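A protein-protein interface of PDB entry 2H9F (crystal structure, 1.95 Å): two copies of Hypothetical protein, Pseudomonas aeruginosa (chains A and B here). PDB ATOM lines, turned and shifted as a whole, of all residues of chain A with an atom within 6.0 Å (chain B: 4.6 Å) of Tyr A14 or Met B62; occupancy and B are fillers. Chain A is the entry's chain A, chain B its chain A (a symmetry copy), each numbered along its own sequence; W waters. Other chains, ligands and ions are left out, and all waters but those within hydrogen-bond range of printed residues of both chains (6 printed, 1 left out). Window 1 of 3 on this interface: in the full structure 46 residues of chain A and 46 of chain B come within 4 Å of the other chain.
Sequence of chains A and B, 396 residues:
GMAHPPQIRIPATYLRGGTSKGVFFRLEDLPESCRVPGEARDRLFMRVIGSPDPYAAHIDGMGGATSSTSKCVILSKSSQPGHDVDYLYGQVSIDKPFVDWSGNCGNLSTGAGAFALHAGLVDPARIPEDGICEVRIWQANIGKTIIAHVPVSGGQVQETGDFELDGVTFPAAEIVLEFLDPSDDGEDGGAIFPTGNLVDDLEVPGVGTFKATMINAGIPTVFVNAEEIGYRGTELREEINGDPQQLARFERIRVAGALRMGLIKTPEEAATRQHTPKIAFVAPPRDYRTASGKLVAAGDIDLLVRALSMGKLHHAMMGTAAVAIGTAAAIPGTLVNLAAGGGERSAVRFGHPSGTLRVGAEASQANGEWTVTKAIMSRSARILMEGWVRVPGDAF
The side-chain amino group (NZ) of Lys A21 sits at hydrogen-bond distance from the backbone carbonyl oxygen (O) of Gly B61 (2.9 Å). NZ of Lys A21 sits at hydrogen-bond distance from O of Gly B63, at 2.9 Å.
The side-chain hydroxyl (OH) of Tyr A14 lies close to the side-chain amino group (NZ) of Lys A21, at 3.4 Å. The backbone NH (N) of Leu A384 sits at hydrogen-bond distance from the backbone carbonyl oxygen (O) of Tyr A14. N of Tyr A14 sits at hydrogen-bond distance from O of Met A385, at 2.8 Å. N of Tyr B14 is in hydrogen-bond range of O of Met B385. The backbone carbonyl oxygen (O) of Val B48 is in hydrogen-bond range of the backbone NH (N) of Met B62 (2.7 Å). The backbone carbonyl oxygen (O) of Ile B49 is in hydrogen-bond range of the backbone NH (N) of Met B62 (3.2 Å).
Among the printed residues, pairs that only touch across the chains: Leu A384 with Val B389, Ala A12 with Met B385, Met A385 with Met B385, Leu A384 with Gly B61, Glu A386 with Met B385, Met A62 with Met B385, Met A385 with Met B62, Tyr A14 with Met B62, Met A62 with Tyr B14, Met A385 with Tyr B14, Tyr A14 with Met B385 and Leu A384 with Met B62.
Of the printed residues of chain B, Ala A12 touches Met B385 (3.4 Å). Of the printed residues of chain B, Tyr A14 touches Met B62 and Met B385. Arg A382 touches none of the printed residues of chain B. Ile A383 touches none of the printed residues of chain B. Of the printed residues of chain B, Leu A384 touches Gly B61 (3.7 Å), Met B62 (3.97 Å) and Val B389 (3.4 Å). Of chain A, only Tyr A14, Leu A384 and Met A385 come within 4 Å of Met B62. Of the printed residues of chain A, Gly B63 touches Lys A21. Printed residues of chain A within 4 Å of Val B389: Leu A384 (3.4 Å). The nearest printed residue of chain B that does not touch Tyr A14 is Gly B61 (4.6 Å). The nearest printed residue of chain B that does not touch Met A385 is Val B389 (4.1 Å).
Hydrophobic or aromatic side chains of chain B within 4 Å of the printed part of chain A: Tyr B14, Met B62, Met B385 and Val B389. Of the 18 printed residues of chain A, 7 touch a printed residue of chain B. Hydrophobic or aromatic side chains of chain A within 4 Å of the printed part of chain B: Tyr A14, Met A62, Leu A384 and Met A385. Among the printed residues, 14 pairs touch across the chains.
Tyr A14 touches Met B62, and with the chains exchanged Met A62 touches Tyr B14. Tyr A14 touches Met B385, and with the chains exchanged Met A385 touches Tyr B14. Met A62 touches Met B385, and with the chains exchanged Met A385 touches Met B62. Met A385 touches its own counterpart, Met B385.
Water W2 lies within hydrogen-bond range of the backbone carbonyl oxygen of Gly B64 (2.7 Å) and the backbone carbonyl oxygen of Gly A64 (3.1 Å). Water W3 lies within hydrogen-bond range of O of Gly A64 (2.7 Å) and O of Gly B64 (3.1 Å). Water W4 lies within hydrogen-bond range of O of Met B62 (2.7 Å), OH of Tyr A14 (3.1 Å) and NZ of Lys A21 (3.2 Å). Water W1 bridges the backbone carbonyl oxygen of Met A62 and the side-chain hydroxyl of Tyr B14. Water W5 lies within hydrogen-bond range of NH2 of Arg A382 (3.1 Å) and O of Val B48 (3.2 Å). Water W6 lies within hydrogen-bond range of NZ of Lys A21 (3.2 Å) and O of Gly B63 (3.3 Å).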
ATOM      1  N   ALA A  12      25.361  12.454 -29.020  1.00  0.00           N
ATOM      2  CA  ALA A  12      24.830  12.451 -27.656  1.00  0.00           C
ATOM      3  C   ALA A  12      25.097  11.083 -27.062  1.00  0.00           C
ATOM      4  O   ALA A  12      25.285  10.115 -27.781  1.00  0.00           O
ATOM      5  CB  ALA A  12      23.299  12.662 -27.603  1.00  0.00           C
ATOM      6  N   THR A  13      25.014  11.060 -25.744  1.00  0.00           N
ATOM      7  CA  THR A  13      25.118   9.863 -24.932  1.00  0.00           C
ATOM      8  C   THR A  13      23.980   9.900 -23.912  1.00  0.00           C
ATOM      9  O   THR A  13      23.741  10.914 -23.211  1.00  0.00           O
ATOM     10  CB  THR A  13      26.478   9.785 -24.265  1.00  0.00           C
ATOM     11  OG1 THR A  13      27.476   9.988 -25.281  1.00  0.00           O
ATOM     12  CG2 THR A  13      26.690   8.396 -23.587  1.00  0.00           C
ATOM     13  N   TYR A  14      23.282   8.775 -23.835  1.00  0.00           N
ATOM     14  CA  TYR A  14      22.185   8.657 -22.917  1.00  0.00           C
ATOM     15  C   TYR A  14      22.646   7.782 -21.766  1.00  0.00           C
ATOM     16  O   TYR A  14      23.001   6.616 -21.954  1.00  0.00           O
ATOM     17  CB  TYR A  14      20.977   8.094 -23.657  1.00  0.00           C
ATOM     18  CG  TYR A  14      19.688   8.034 -22.875  1.00  0.00           C
ATOM     19  CD1 TYR A  14      19.128   9.158 -22.299  1.00  0.00           C
ATOM     20  CD2 TYR A  14      19.030   6.842 -22.707  1.00  0.00           C
ATOM     21  CE1 TYR A  14      17.903   9.106 -21.585  1.00  0.00           C
ATOM     22  CE2 TYR A  14      17.816   6.777 -22.001  1.00  0.00           C
ATOM     23  CZ  TYR A  14      17.280   7.880 -21.430  1.00  0.00           C
ATOM     24  OH  TYR A  14      16.112   7.765 -20.752  1.00  0.00           O
ATOM     25  N   LEU A  15      22.685   8.377 -20.580  1.00  0.00           N
ATOM     26  CA  LEU A  15      23.267   7.713 -19.402  1.00  0.00           C
ATOM     27  C   LEU A  15      22.268   7.702 -18.269  1.00  0.00           C
ATOM     28  O   LEU A  15      21.485   8.659 -18.078  1.00  0.00           O
ATOM     29  CB  LEU A  15      24.449   8.500 -18.813  1.00  0.00           C
ATOM     30  CG  LEU A  15      25.789   8.601 -19.514  1.00  0.00           C
ATOM     31  CD1 LEU A  15      25.893   9.912 -20.182  1.00  0.00           C
ATOM     32  CD2 LEU A  15      26.938   8.417 -18.481  1.00  0.00           C
ATOM     33  N   ARG A  16      22.394   6.667 -17.454  1.00  0.00           N
ATOM     34  CA  ARG A  16      21.881   6.669 -16.102  1.00  0.00           C
ATOM     35  C   ARG A  16      22.945   7.198 -15.180  1.00  0.00           C
ATOM     36  O   ARG A  16      24.067   6.697 -15.171  1.00  0.00           O
ATOM     37  CB  ARG A  16      21.552   5.279 -15.607  1.00  0.00           C
ATOM     38  CG  ARG A  16      21.038   5.324 -14.177  1.00  0.00           C
ATOM     39  CD  ARG A  16      20.765   3.971 -13.559  1.00  0.00           C
ATOM     40  NE  ARG A  16      21.920   3.057 -13.511  1.00  0.00           N
ATOM     41  CZ  ARG A  16      22.929   3.157 -12.648  1.00  0.00           C
ATOM     42  NH1 ARG A  16      22.995   4.164 -11.795  1.00  0.00           N
ATOM     43  NH2 ARG A  16      23.890   2.260 -12.684  1.00  0.00           N
ATOM     44  N   LYS A  21      17.953   9.461 -15.388  1.00  0.00           N
ATOM     45  CA  LYS A  21      18.478   9.287 -16.755  1.00  0.00           C
ATOM     46  C   LYS A  21      18.562  10.676 -17.378  1.00  0.00           C
ATOM     47  O   LYS A  21      17.697  11.500 -17.166  1.00  0.00           O
ATOM     48  CB  LYS A  21      17.582   8.401 -17.604  1.00  0.00           C
ATOM     49  CG  LYS A  21      17.573   6.965 -17.139  1.00  0.00           C
ATOM     50  CD  LYS A  21      16.886   6.008 -18.138  1.00  0.00           C
ATOM     51  CE  LYS A  21      15.330   6.085 -18.164  1.00  0.00           C
ATOM     52  NZ  LYS A  21      14.765   5.129 -19.120  1.00  0.00           N
ATOM     53  N   GLY A  22      19.592  10.913 -18.176  1.00  0.00           N
ATOM     54  CA  GLY A  22      19.729  12.174 -18.874  1.00  0.00           C
ATOM     55  C   GLY A  22      20.401  11.976 -20.234  1.00  0.00           C
ATOM     56  O   GLY A  22      21.068  10.968 -20.478  1.00  0.00           O
ATOM     57  N   VAL A  23      20.198  12.953 -21.112  1.00  0.00           N
ATOM     58  CA  VAL A  23      20.817  12.958 -22.404  1.00  0.00           C
ATOM     59  C   VAL A  23      21.977  13.913 -22.254  1.00  0.00           C
ATOM     60  O   VAL A  23      21.758  15.050 -21.865  1.00  0.00           O
ATOM     61  CB  VAL A  23      19.898  13.478 -23.540  1.00  0.00           C
ATOM     62  CG1 VAL A  23      20.628  13.347 -24.878  1.00  0.00           C
ATOM     63  CG2 VAL A  23      18.550  12.744 -23.580  1.00  0.00           C
ATOM     64  N   PHE A  24      23.194  13.413 -22.525  1.00  0.00           N
ATOM     65  CA  PHE A  24      24.423  14.153 -22.334  1.00  0.00           C
ATOM     66  C   PHE A  24      25.054  14.594 -23.665  1.00  0.00           C
ATOM     67  O   PHE A  24      25.156  13.829 -24.625  1.00  0.00           O
ATOM     68  CB  PHE A  24      25.441  13.336 -21.526  1.00  0.00           C
ATOM     69  CG  PHE A  24      25.141  13.232 -20.064  1.00  0.00           C
ATOM     70  CD1 PHE A  24      24.046  12.505 -19.602  1.00  0.00           C
ATOM     71  CD2 PHE A  24      26.003  13.769 -19.143  1.00  0.00           C
ATOM     72  CE1 PHE A  24      23.780  12.390 -18.269  1.00  0.00           C
ATOM     73  CE2 PHE A  24      25.754  13.643 -17.803  1.00  0.00           C
ATOM     74  CZ  PHE A  24      24.641  12.961 -17.363  1.00  0.00           C
ATOM     75  N   MET A  62      13.107  11.767 -26.026  1.00  0.00           N
ATOM     76  CA  MET A  62      14.020  10.934 -25.233  1.00  0.00           C
ATOM     77  C   MET A  62      13.554  10.865 -23.770  1.00  0.00           C
ATOM     78  O   MET A  62      13.986   9.978 -23.007  1.00  0.00           O
ATOM     79  CB  MET A  62      15.467  11.436 -25.318  1.00  0.00           C
ATOM     80  CG  MET A  62      16.085  11.359 -26.761  1.00  0.00           C
ATOM     81  SD  MET A  62      16.099   9.405 -27.208  1.00  0.00           S
ATOM     82  CE  MET A  62      17.084   8.696 -25.687  1.00  0.00           C
ATOM     83  N   GLY A  63      12.666  11.785 -23.387  1.00  0.00           N
ATOM     84  CA  GLY A  63      12.133  11.838 -22.035  1.00  0.00           C
ATOM     85  C   GLY A  63      11.381  10.573 -21.647  1.00  0.00           C
ATOM     86  O   GLY A  63      11.006   9.731 -22.486  1.00  0.00           O
ATOM     87  N   GLY A  64      11.184  10.412 -20.345  1.00  0.00           N
ATOM     88  CA  GLY A  64      10.366   9.311 -19.826  1.00  0.00           C
ATOM     89  C   GLY A  64       9.165   9.827 -19.040  1.00  0.00           C
ATOM     90  O   GLY A  64       8.573   9.091 -18.283  1.00  0.00           O
ATOM     91  N   THR A  69      13.559  11.702 -15.501  1.00  0.00           N
ATOM     92  CA  THR A  69      13.865  11.284 -16.858  1.00  0.00           C
ATOM     93  C   THR A  69      13.565  12.393 -17.824  1.00  0.00           C
ATOM     94  O   THR A  69      13.230  12.129 -18.968  1.00  0.00           O
ATOM     95  CB  THR A  69      13.033  10.052 -17.291  1.00  0.00           C
ATOM     96  OG1 THR A  69      11.633  10.367 -17.178  1.00  0.00           O
ATOM     97  CG2 THR A  69      13.363   8.847 -16.473  1.00  0.00           C
ATOM     98  N   ARG A 382      25.930   4.501 -15.694  1.00  0.00           N
ATOM     99  CA  ARG A 382      26.293   3.744 -16.877  1.00  0.00           C
ATOM    100  C   ARG A 382      25.665   4.308 -18.143  1.00  0.00           C
ATOM    101  O   ARG A 382      24.568   4.917 -18.125  1.00  0.00           O
ATOM    102  CB  ARG A 382      25.896   2.254 -16.755  1.00  0.00           C
ATOM    103  CG  ARG A 382      24.466   1.996 -16.542  1.00  0.00           C
ATOM    104  CD  ARG A 382      24.171   0.452 -16.366  1.00  0.00           C
ATOM    105  NE  ARG A 382      24.062  -0.163 -17.636  1.00  0.00           N
ATOM    106  CZ  ARG A 382      22.937  -0.481 -18.265  1.00  0.00           C
ATOM    107  NH1 ARG A 382      21.727  -0.338 -17.753  1.00  0.00           N
ATOM    108  NH2 ARG A 382      23.047  -1.028 -19.451  1.00  0.00           N
ATOM    109  N   ILE A 383      26.372   4.097 -19.250  1.00  0.00           N
ATOM    110  CA  ILE A 383      25.865   4.439 -20.562  1.00  0.00           C
ATOM    111  C   ILE A 383      24.783   3.457 -20.971  1.00  0.00           C
ATOM    112  O   ILE A 383      24.977   2.231 -20.894  1.00  0.00           O
ATOM    113  CB  ILE A 383      27.013   4.502 -21.629  1.00  0.00           C
ATOM    114  CG1 ILE A 383      27.881   5.746 -21.379  1.00  0.00           C
ATOM    115  CG2 ILE A 383      26.411   4.570 -23.064  1.00  0.00           C
ATOM    116  CD1 ILE A 383      29.166   5.749 -22.243  1.00  0.00           C
ATOM    117  N   LEU A 384      23.646   3.987 -21.403  1.00  0.00           N
ATOM    118  CA  LEU A 384      22.533   3.152 -21.878  1.00  0.00           C
ATOM    119  C   LEU A 384      22.532   3.092 -23.413  1.00  0.00           C
ATOM    120  O   LEU A 384      22.302   2.077 -24.018  1.00  0.00           O
ATOM    121  CB  LEU A 384      21.188   3.758 -21.369  1.00  0.00           C
ATOM    122  CG  LEU A 384      21.049   3.926 -19.839  1.00  0.00           C
ATOM    123  CD1 LEU A 384      19.760   4.614 -19.443  1.00  0.00           C
ATOM    124  CD2 LEU A 384      21.174   2.632 -19.157  1.00  0.00           C
ATOM    125  N   MET A 385      22.743   4.238 -24.043  1.00  0.00           N
ATOM    126  CA  MET A 385      22.863   4.289 -25.474  1.00  0.00           C
ATOM    127  C   MET A 385      23.784   5.445 -25.879  1.00  0.00           C
ATOM    128  O   MET A 385      23.843   6.434 -25.199  1.00  0.00           O
ATOM    129  CB  MET A 385      21.440   4.406 -26.085  1.00  0.00           C
ATOM    130  CG  MET A 385      21.421   4.239 -27.596  1.00  0.00           C
ATOM    131  SD  MET A 385      19.609   4.244 -28.326  1.00  0.00           S
ATOM    132  CE  MET A 385      20.130   3.909 -30.076  1.00  0.00           C
ATOM    133  N   GLU A 386      24.535   5.276 -26.964  1.00  0.00           N
ATOM    134  CA  GLU A 386      25.421   6.307 -27.460  1.00  0.00           C
ATOM    135  C   GLU A 386      25.313   6.407 -28.987  1.00  0.00           C
ATOM    136  O   GLU A 386      25.075   5.444 -29.655  1.00  0.00           O
ATOM    137  CB  GLU A 386      26.865   5.967 -27.095  1.00  0.00           C
ATOM    138  CG  GLU A 386      27.243   4.548 -27.538  1.00  0.00           C
ATOM    139  CD  GLU A 386      28.705   4.193 -27.361  1.00  0.00           C
ATOM    140  OE1 GLU A 386      29.591   4.932 -27.833  1.00  0.00           O
ATOM    141  OE2 GLU A 386      28.956   3.144 -26.767  1.00  0.00           O
ATOM    142  N   TYR B  14      16.589   3.676 -31.844  1.00  0.00           N
ATOM    143  CA  TYR B  14      15.468   3.897 -30.976  1.00  0.00           C
ATOM    144  C   TYR B  14      14.492   4.796 -31.711  1.00  0.00           C
ATOM    145  O   TYR B  14      14.816   5.931 -32.070  1.00  0.00           O
ATOM    146  CB  TYR B  14      15.968   4.493 -29.664  1.00  0.00           C
ATOM    147  CG  TYR B  14      14.936   4.661 -28.575  1.00  0.00           C
ATOM    148  CD1 TYR B  14      14.193   3.598 -28.102  1.00  0.00           C
ATOM    149  CD2 TYR B  14      14.700   5.894 -28.024  1.00  0.00           C
ATOM    150  CE1 TYR B  14      13.241   3.751 -27.060  1.00  0.00           C
ATOM    151  CE2 TYR B  14      13.759   6.060 -26.992  1.00  0.00           C
ATOM    152  CZ  TYR B  14      13.027   5.015 -26.541  1.00  0.00           C
ATOM    153  OH  TYR B  14      12.126   5.227 -25.551  1.00  0.00           O
ATOM    154  N   VAL B  23      13.047  -0.194 -29.226  1.00  0.00           N
ATOM    155  CA  VAL B  23      14.437  -0.292 -29.554  1.00  0.00           C
ATOM    156  C   VAL B  23      14.482  -1.303 -30.676  1.00  0.00           C
ATOM    157  O   VAL B  23      13.992  -2.407 -30.494  1.00  0.00           O
ATOM    158  CB  VAL B  23      15.323  -0.811 -28.392  1.00  0.00           C
ATOM    159  CG1 VAL B  23      16.790  -0.782 -28.825  1.00  0.00           C
ATOM    160  CG2 VAL B  23      15.119  -0.005 -27.102  1.00  0.00           C
ATOM    161  N   VAL B  48      18.221  -4.705 -22.012  1.00  0.00           N
ATOM    162  CA  VAL B  48      18.221  -3.419 -22.779  1.00  0.00           C
ATOM    163  C   VAL B  48      17.156  -2.504 -22.249  1.00  0.00           C
ATOM    164  O   VAL B  48      17.353  -1.253 -22.117  1.00  0.00           O
ATOM    165  CB  VAL B  48      18.008  -3.699 -24.304  1.00  0.00           C
ATOM    166  CG1 VAL B  48      17.568  -2.478 -25.070  1.00  0.00           C
ATOM    167  CG2 VAL B  48      19.306  -4.277 -24.890  1.00  0.00           C
ATOM    168  N   ILE B  49      15.983  -3.090 -22.040  1.00  0.00           N
ATOM    169  CA  ILE B  49      14.816  -2.376 -21.519  1.00  0.00           C
ATOM    170  C   ILE B  49      14.911  -1.918 -20.065  1.00  0.00           C
ATOM    171  O   ILE B  49      14.466  -0.789 -19.731  1.00  0.00           O
ATOM    172  CB  ILE B  49      13.513  -3.161 -21.750  1.00  0.00           C
ATOM    173  CG1 ILE B  49      13.172  -3.133 -23.254  1.00  0.00           C
ATOM    174  CG2 ILE B  49      12.350  -2.576 -20.946  1.00  0.00           C
ATOM    175  CD1 ILE B  49      13.074  -1.724 -23.869  1.00  0.00           C
ATOM    176  N   GLY B  50      15.594  -2.715 -19.261  1.00  0.00           N
ATOM    177  CA  GLY B  50      15.829  -2.408 -17.851  1.00  0.00           C
ATOM    178  C   GLY B  50      14.936  -3.216 -16.922  1.00  0.00           C
ATOM    179  O   GLY B  50      14.657  -2.775 -15.795  1.00  0.00           O
ATOM    180  N   GLY B  61      17.507   1.353 -17.847  1.00  0.00           N
ATOM    181  CA  GLY B  61      17.401   0.826 -19.178  1.00  0.00           C
ATOM    182  C   GLY B  61      16.673   1.719 -20.123  1.00  0.00           C
ATOM    183  O   GLY B  61      16.432   2.934 -19.848  1.00  0.00           O
ATOM    184  N   MET B  62      16.414   1.165 -21.312  1.00  0.00           N
ATOM    185  CA  MET B  62      15.879   1.980 -22.410  1.00  0.00           C
ATOM    186  C   MET B  62      14.358   2.142 -22.271  1.00  0.00           C
ATOM    187  O   MET B  62      13.754   3.037 -22.895  1.00  0.00           O
ATOM    188  CB  MET B  62      16.239   1.394 -23.781  1.00  0.00           C
ATOM    189  CG  MET B  62      17.782   1.371 -24.080  1.00  0.00           C
ATOM    190  SD  MET B  62      18.332   3.299 -24.086  1.00  0.00           S
ATOM    191  CE  MET B  62      17.094   4.019 -25.405  1.00  0.00           C
ATOM    192  N   GLY B  63      13.744   1.291 -21.444  1.00  0.00           N
ATOM    193  CA  GLY B  63      12.310   1.330 -21.210  1.00  0.00           C
ATOM    194  C   GLY B  63      11.844   2.651 -20.616  1.00  0.00           C
ATOM    195  O   GLY B  63      12.631   3.474 -20.109  1.00  0.00           O
ATOM    196  N   GLY B  64      10.541   2.882 -20.709  1.00  0.00           N
ATOM    197  CA  GLY B  64       9.924   4.049 -20.071  1.00  0.00           C
ATOM    198  C   GLY B  64       8.875   3.639 -19.044  1.00  0.00           C
ATOM    199  O   GLY B  64       8.053   4.440 -18.660  1.00  0.00           O
ATOM    200  N   MET B 385      16.933   8.222 -31.480  1.00  0.00           N
ATOM    201  CA  MET B 385      18.353   8.100 -31.289  1.00  0.00           C
ATOM    202  C   MET B 385      18.877   6.877 -32.050  1.00  0.00           C
ATOM    203  O   MET B 385      18.170   5.918 -32.207  1.00  0.00           O
ATOM    204  CB  MET B 385      18.642   8.036 -29.765  1.00  0.00           C
ATOM    205  CG  MET B 385      20.122   8.135 -29.432  1.00  0.00           C
ATOM    206  SD  MET B 385      20.452   8.199 -27.507  1.00  0.00           S
ATOM    207  CE  MET B 385      22.289   8.423 -27.658  1.00  0.00           C
ATOM    208  N   VAL B 389      23.285   0.472 -28.192  1.00  0.00           N
ATOM    209  CA  VAL B 389      22.916   0.275 -26.807  1.00  0.00           C
ATOM    210  C   VAL B 389      24.054  -0.456 -26.108  1.00  0.00           C
ATOM    211  O   VAL B 389      24.766  -1.275 -26.730  1.00  0.00           O
ATOM    212  CB  VAL B 389      21.580  -0.490 -26.615  1.00  0.00           C
ATOM    213  CG1 VAL B 389      20.426   0.298 -27.048  1.00  0.00           C
ATOM    214  CG2 VAL B 389      21.559  -1.914 -27.325  1.00  0.00           C
HETATM  215  O   HOH W   1      13.328   7.413 -23.713  1.00  0.00           O
HETATM  216  O   HOH W   2       7.365   6.736 -19.961  1.00  0.00           O
HETATM  217  O   HOH W   3       9.569   6.781 -17.230  1.00  0.00           O
HETATM  218  O   HOH W   4      14.448   5.600 -22.219  1.00  0.00           O
HETATM  219  O   HOH W   5      20.123  -1.122 -20.493  1.00  0.00           O
HETATM  220  O   HOH W   6      12.040   5.505 -17.556  1.00  0.00           O
